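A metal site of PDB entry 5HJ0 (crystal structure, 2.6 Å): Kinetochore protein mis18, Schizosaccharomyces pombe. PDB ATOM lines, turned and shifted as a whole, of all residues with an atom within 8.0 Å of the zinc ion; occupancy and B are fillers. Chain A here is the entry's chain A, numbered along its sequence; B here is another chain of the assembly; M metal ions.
N of Lys 27 sits close to SG of Cys 25, 3.4 Å away. N of Cys 25 sits at hydrogen-bond distance from O of Gln 30 (2.9 Å). SG of Cys 28 lies close to N of Gln 30 (3.6 Å). The side-chain sulfur of Cys 79 sits close to the backbone NH of Arg 81 (3.3 Å). O of Glu 84 is in hydrogen-bond range of N of Cys 79, 2.9 Å away. The side-chain sulfur (SG) of Cys 79 sits close to the side-chain amide oxygen (OE1) of Gln 30 (3.7 Å).
Of the 21 residues printed, 4 come within 4 Å of the zinc ion.
The zinc ion is bound by SG of Cys 82 (2.3 Å), SG of Cys 25 (2.3 Å), SG of Cys 28 (2.3 Å) and SG of Cys 79 (2.4 Å). The zinc ion has four donor atoms within binding distance.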
ATOM      1  N   GLN A  24      -5.491  -2.416  33.652  1.00  0.00           N
ATOM      2  CA  GLN A  24      -4.918  -1.140  33.298  1.00  0.00           C
ATOM      3  C   GLN A  24      -3.506  -1.329  32.823  1.00  0.00           C
ATOM      4  O   GLN A  24      -2.761  -2.132  33.396  1.00  0.00           O
ATOM      5  CB  GLN A  24      -4.840  -0.223  34.521  1.00  0.00           C
ATOM      6  CG  GLN A  24      -6.133   0.373  35.010  1.00  0.00           C
ATOM      7  CD  GLN A  24      -5.907   1.159  36.293  1.00  0.00           C
ATOM      8  OE1 GLN A  24      -5.576   0.589  37.335  1.00  0.00           O
ATOM      9  NE2 GLN A  24      -6.096   2.474  36.228  1.00  0.00           N
ATOM     10  N   CYS A  25      -3.126  -0.550  31.824  1.00  0.00           N
ATOM     11  CA  CYS A  25      -1.731  -0.365  31.542  1.00  0.00           C
ATOM     12  C   CYS A  25      -1.026   0.166  32.816  1.00  0.00           C
ATOM     13  O   CYS A  25      -1.552   1.041  33.503  1.00  0.00           O
ATOM     14  CB  CYS A  25      -1.554   0.588  30.361  1.00  0.00           C
ATOM     15  SG  CYS A  25       0.132   1.091  30.103  1.00  0.00           S
ATOM     16  N   LYS A  26       0.111  -0.432  33.132  1.00  0.00           N
ATOM     17  CA  LYS A  26       0.939  -0.089  34.295  1.00  0.00           C
ATOM     18  C   LYS A  26       1.572   1.304  34.215  1.00  0.00           C
ATOM     19  O   LYS A  26       1.812   1.909  35.269  1.00  0.00           O
ATOM     20  CB  LYS A  26       2.069  -1.102  34.444  1.00  0.00           C
ATOM     21  CG  LYS A  26       1.854  -2.150  35.515  1.00  0.00           C
ATOM     22  CD  LYS A  26       3.132  -2.967  35.699  1.00  0.00           C
ATOM     23  CE  LYS A  26       3.547  -3.055  37.169  1.00  0.00           C
ATOM     24  NZ  LYS A  26       2.631  -3.874  38.028  1.00  0.00           N
ATOM     25  N   LYS A  27       1.845   1.787  32.995  1.00  0.00           N
ATOM     26  CA  LYS A  27       2.624   3.015  32.784  1.00  0.00           C
ATOM     27  C   LYS A  27       1.788   4.285  32.909  1.00  0.00           C
ATOM     28  O   LYS A  27       1.913   5.047  33.869  1.00  0.00           O
ATOM     29  CB  LYS A  27       3.343   2.985  31.423  1.00  0.00           C
ATOM     30  CG  LYS A  27       4.763   2.485  31.463  1.00  0.00           C
ATOM     31  CD  LYS A  27       5.762   3.630  31.657  1.00  0.00           C
ATOM     32  CE  LYS A  27       6.771   3.329  32.773  1.00  0.00           C
ATOM     33  NZ  LYS A  27       7.398   1.964  32.715  1.00  0.00           N
ATOM     34  N   CYS A  28       0.982   4.508  31.861  1.00  0.00           N
ATOM     35  CA  CYS A  28      -0.148   5.426  31.825  1.00  0.00           C
ATOM     36  C   CYS A  28      -1.207   4.562  32.459  1.00  0.00           C
ATOM     37  O   CYS A  28      -0.969   3.356  32.618  1.00  0.00           O
ATOM     38  CB  CYS A  28      -0.485   5.692  30.356  1.00  0.00           C
ATOM     39  SG  CYS A  28      -1.455   4.394  29.532  1.00  0.00           S
ATOM     40  N   PHE A  29      -2.366   5.081  32.846  1.00  0.00           N
ATOM     41  CA  PHE A  29      -3.214   4.113  33.569  1.00  0.00           C
ATOM     42  C   PHE A  29      -4.478   3.655  32.845  1.00  0.00           C
ATOM     43  O   PHE A  29      -5.496   3.328  33.475  1.00  0.00           O
ATOM     44  CB  PHE A  29      -3.405   4.533  35.024  1.00  0.00           C
ATOM     45  CG  PHE A  29      -2.154   4.437  35.823  1.00  0.00           C
ATOM     46  CD1 PHE A  29      -1.298   5.546  35.949  1.00  0.00           C
ATOM     47  CD2 PHE A  29      -1.787   3.243  36.438  1.00  0.00           C
ATOM     48  CE1 PHE A  29      -0.115   5.461  36.681  1.00  0.00           C
ATOM     49  CE2 PHE A  29      -0.606   3.136  37.168  1.00  0.00           C
ATOM     50  CZ  PHE A  29       0.231   4.256  37.290  1.00  0.00           C
ATOM     51  N   GLN A  30      -4.364   3.602  31.523  1.00  0.00           N
ATOM     52  CA  GLN A  30      -5.483   3.390  30.640  1.00  0.00           C
ATOM     53  C   GLN A  30      -6.045   2.006  30.811  1.00  0.00           C
ATOM     54  O   GLN A  30      -5.292   1.029  30.828  1.00  0.00           O
ATOM     55  CB  GLN A  30      -5.071   3.616  29.196  1.00  0.00           C
ATOM     56  CG  GLN A  30      -6.221   3.595  28.215  1.00  0.00           C
ATOM     57  CD  GLN A  30      -5.832   4.240  26.914  1.00  0.00           C
ATOM     58  OE1 GLN A  30      -5.036   3.675  26.147  1.00  0.00           O
ATOM     59  NE2 GLN A  30      -6.341   5.432  26.661  1.00  0.00           N
ATOM     60  N   ILE A  31      -7.365   1.963  30.978  1.00  0.00           N
ATOM     61  CA  ILE A  31      -8.135   0.717  31.121  1.00  0.00           C
ATOM     62  C   ILE A  31      -8.212   0.013  29.757  1.00  0.00           C
ATOM     63  O   ILE A  31      -8.756   0.578  28.810  1.00  0.00           O
ATOM     64  CB  ILE A  31      -9.540   0.994  31.733  1.00  0.00           C
ATOM     65  CG1 ILE A  31      -9.392   1.390  33.209  1.00  0.00           C
ATOM     66  CG2 ILE A  31     -10.464  -0.206  31.581  1.00  0.00           C
ATOM     67  CD1 ILE A  31     -10.656   1.874  33.883  1.00  0.00           C
ATOM     68  N   VAL A  32      -7.662  -1.199  29.682  1.00  0.00           N
ATOM     69  CA  VAL A  32      -7.584  -1.952  28.420  1.00  0.00           C
ATOM     70  C   VAL A  32      -8.774  -2.885  28.222  1.00  0.00           C
ATOM     71  O   VAL A  32      -9.140  -3.224  27.097  1.00  0.00           O
ATOM     72  CB  VAL A  32      -6.259  -2.731  28.285  1.00  0.00           C
ATOM     73  CG1 VAL A  32      -5.085  -1.773  28.301  1.00  0.00           C
ATOM     74  CG2 VAL A  32      -6.122  -3.769  29.384  1.00  0.00           C
ATOM     75  N   SER A  57      -8.326   1.811  23.423  1.00  0.00           N
ATOM     76  CA  SER A  57      -7.225   1.729  24.383  1.00  0.00           C
ATOM     77  C   SER A  57      -6.064   0.894  23.887  1.00  0.00           C
ATOM     78  O   SER A  57      -4.965   0.972  24.414  1.00  0.00           O
ATOM     79  CB  SER A  57      -7.741   1.233  25.725  1.00  0.00           C
ATOM     80  OG  SER A  57      -8.671   2.178  26.223  1.00  0.00           O
ATOM     81  N   SER A  78      -0.265  -2.789  21.368  1.00  0.00           N
ATOM     82  CA  SER A  78       0.267  -1.664  22.093  1.00  0.00           C
ATOM     83  C   SER A  78      -0.850  -0.889  22.742  1.00  0.00           C
ATOM     84  O   SER A  78      -1.976  -0.838  22.206  1.00  0.00           O
ATOM     85  CB  SER A  78       1.033  -0.739  21.141  1.00  0.00           C
ATOM     86  OG  SER A  78       2.117  -1.432  20.525  1.00  0.00           O
ATOM     87  N   CYS A  79      -0.553  -0.323  23.927  1.00  0.00           N
ATOM     88  CA  CYS A  79      -1.389   0.673  24.574  1.00  0.00           C
ATOM     89  C   CYS A  79      -1.427   1.922  23.722  1.00  0.00           C
ATOM     90  O   CYS A  79      -0.403   2.428  23.289  1.00  0.00           O
ATOM     91  CB  CYS A  79      -0.872   1.027  25.980  1.00  0.00           C
ATOM     92  SG  CYS A  79      -1.563   2.511  26.792  1.00  0.00           S
ATOM     93  N   THR A  80      -2.625   2.415  23.505  1.00  0.00           N
ATOM     94  CA  THR A  80      -2.870   3.622  22.740  1.00  0.00           C
ATOM     95  C   THR A  80      -2.303   4.892  23.351  1.00  0.00           C
ATOM     96  O   THR A  80      -1.854   5.776  22.620  1.00  0.00           O
ATOM     97  CB  THR A  80      -4.364   3.732  22.527  1.00  0.00           C
ATOM     98  OG1 THR A  80      -4.698   2.885  21.414  1.00  0.00           O
ATOM     99  CG2 THR A  80      -4.831   5.177  22.289  1.00  0.00           C
ATOM    100  N   ARG A  81      -2.303   4.980  24.676  1.00  0.00           N
ATOM    101  CA  ARG A  81      -1.854   6.183  25.360  1.00  0.00           C
ATOM    102  C   ARG A  81      -0.325   6.317  25.409  1.00  0.00           C
ATOM    103  O   ARG A  81       0.207   7.373  25.092  1.00  0.00           O
ATOM    104  CB  ARG A  81      -2.493   6.316  26.752  1.00  0.00           C
ATOM    105  CG  ARG A  81      -2.024   7.526  27.563  1.00  0.00           C
ATOM    106  CD  ARG A  81      -2.782   7.667  28.868  1.00  0.00           C
ATOM    107  NE  ARG A  81      -3.625   8.865  28.893  1.00  0.00           N
ATOM    108  CZ  ARG A  81      -3.551   9.833  29.815  1.00  0.00           C
ATOM    109  NH1 ARG A  81      -2.689   9.774  30.827  1.00  0.00           N
ATOM    110  NH2 ARG A  81      -4.378  10.859  29.715  1.00  0.00           N
ATOM    111  N   CYS A  82       0.377   5.258  25.796  1.00  0.00           N
ATOM    112  CA  CYS A  82       1.815   5.396  26.018  1.00  0.00           C
ATOM    113  C   CYS A  82       2.694   4.528  25.112  1.00  0.00           C
ATOM    114  O   CYS A  82       3.912   4.568  25.230  1.00  0.00           O
ATOM    115  CB  CYS A  82       2.134   5.145  27.493  1.00  0.00           C
ATOM    116  SG  CYS A  82       2.050   3.418  27.918  1.00  0.00           S
ATOM    117  N   ASN A  83       2.034   3.750  24.251  1.00  0.00           N
ATOM    118  CA  ASN A  83       2.666   2.921  23.197  1.00  0.00           C
ATOM    119  C   ASN A  83       3.531   1.782  23.719  1.00  0.00           C
ATOM    120  O   ASN A  83       4.403   1.278  23.011  1.00  0.00           O
ATOM    121  CB  ASN A  83       3.406   3.779  22.155  1.00  0.00           C
ATOM    122  CG  ASN A  83       2.574   4.951  21.671  1.00  0.00           C
ATOM    123  OD1 ASN A  83       1.559   4.784  20.972  1.00  0.00           O
ATOM    124  ND2 ASN A  83       2.995   6.153  22.054  1.00  0.00           N
ATOM    125  N   GLU A  84       3.284   1.368  24.954  1.00  0.00           N
ATOM    126  CA  GLU A  84       3.891   0.167  25.500  1.00  0.00           C
ATOM    127  C   GLU A  84       3.332  -1.036  24.765  1.00  0.00           C
ATOM    128  O   GLU A  84       2.144  -1.087  24.467  1.00  0.00           O
ATOM    129  CB  GLU A  84       3.580   0.050  26.994  1.00  0.00           C
ATOM    130  CG  GLU A  84       4.608  -0.712  27.811  1.00  0.00           C
ATOM    131  CD  GLU A  84       5.985  -0.057  27.825  1.00  0.00           C
ATOM    132  OE1 GLU A  84       6.958  -0.808  28.046  1.00  0.00           O
ATOM    133  OE2 GLU A  84       6.102   1.178  27.610  1.00  0.00           O
ATOM    134  N   VAL A  85       4.198  -2.003  24.461  1.00  0.00           N
ATOM    135  CA  VAL A  85       3.729  -3.294  23.954  1.00  0.00           C
ATOM    136  C   VAL A  85       3.236  -4.085  25.166  1.00  0.00           C
ATOM    137  O   VAL A  85       4.027  -4.488  26.007  1.00  0.00           O
ATOM    138  CB  VAL A  85       4.830  -4.033  23.150  1.00  0.00           C
ATOM    139  CG1 VAL A  85       4.335  -5.396  22.673  1.00  0.00           C
ATOM    140  CG2 VAL A  85       5.257  -3.197  21.954  1.00  0.00           C
ATOM    141  N   ILE A  86       1.914  -4.253  25.266  1.00  0.00           N
ATOM    142  CA  ILE A  86       1.270  -4.826  26.470  1.00  0.00           C
ATOM    143  C   ILE A  86       0.767  -6.256  26.279  1.00  0.00           C
ATOM    144  O   ILE A  86       0.299  -6.894  27.234  1.00  0.00           O
ATOM    145  CB  ILE A  86       0.147  -3.908  27.017  1.00  0.00           C
ATOM    146  CG1 ILE A  86      -0.963  -3.715  25.958  1.00  0.00           C
ATOM    147  CG2 ILE A  86       0.738  -2.597  27.523  1.00  0.00           C
ATOM    148  CD1 ILE A  86      -2.166  -2.906  26.434  1.00  0.00           C
ATOM    149  N   LYS A 110       2.910  -6.225  32.334  1.00  0.00           N
ATOM    150  CA  LYS A 110       2.644  -4.919  31.724  1.00  0.00           C
ATOM    151  C   LYS A 110       1.316  -4.272  32.172  1.00  0.00           C
ATOM    152  O   LYS A 110       1.024  -3.121  31.843  1.00  0.00           O
ATOM    153  CB  LYS A 110       2.674  -5.030  30.191  1.00  0.00           C
ATOM    154  CG  LYS A 110       4.014  -5.452  29.608  1.00  0.00           C
ATOM    155  CD  LYS A 110       5.050  -4.355  29.669  1.00  0.00           C
ATOM    156  CE  LYS A 110       6.287  -4.720  28.882  1.00  0.00           C
ATOM    157  NZ  LYS A 110       7.282  -3.628  29.000  1.00  0.00           N
ATOM    158  N   PHE B  29      -4.635   8.661  34.668  1.00  0.00           N
ATOM    159  CA  PHE B  29      -5.846   7.835  34.567  1.00  0.00           C
ATOM    160  C   PHE B  29      -6.195   7.091  35.875  1.00  0.00           C
ATOM    161  O   PHE B  29      -6.863   6.062  35.829  1.00  0.00           O
ATOM    162  CB  PHE B  29      -5.826   6.895  33.340  1.00  0.00           C
ATOM    163  CG  PHE B  29      -6.415   7.484  32.071  1.00  0.00           C
ATOM    164  CD1 PHE B  29      -7.409   8.467  32.091  1.00  0.00           C
ATOM    165  CD2 PHE B  29      -6.010   7.007  30.816  1.00  0.00           C
ATOM    166  CE1 PHE B  29      -7.957   8.968  30.911  1.00  0.00           C
ATOM    167  CE2 PHE B  29      -6.559   7.505  29.626  1.00  0.00           C
ATOM    168  CZ  PHE B  29      -7.532   8.487  29.678  1.00  0.00           C
HETATM  169 ZN    ZN M   1      -0.051   2.796  28.583  1.00  0.00          ZN
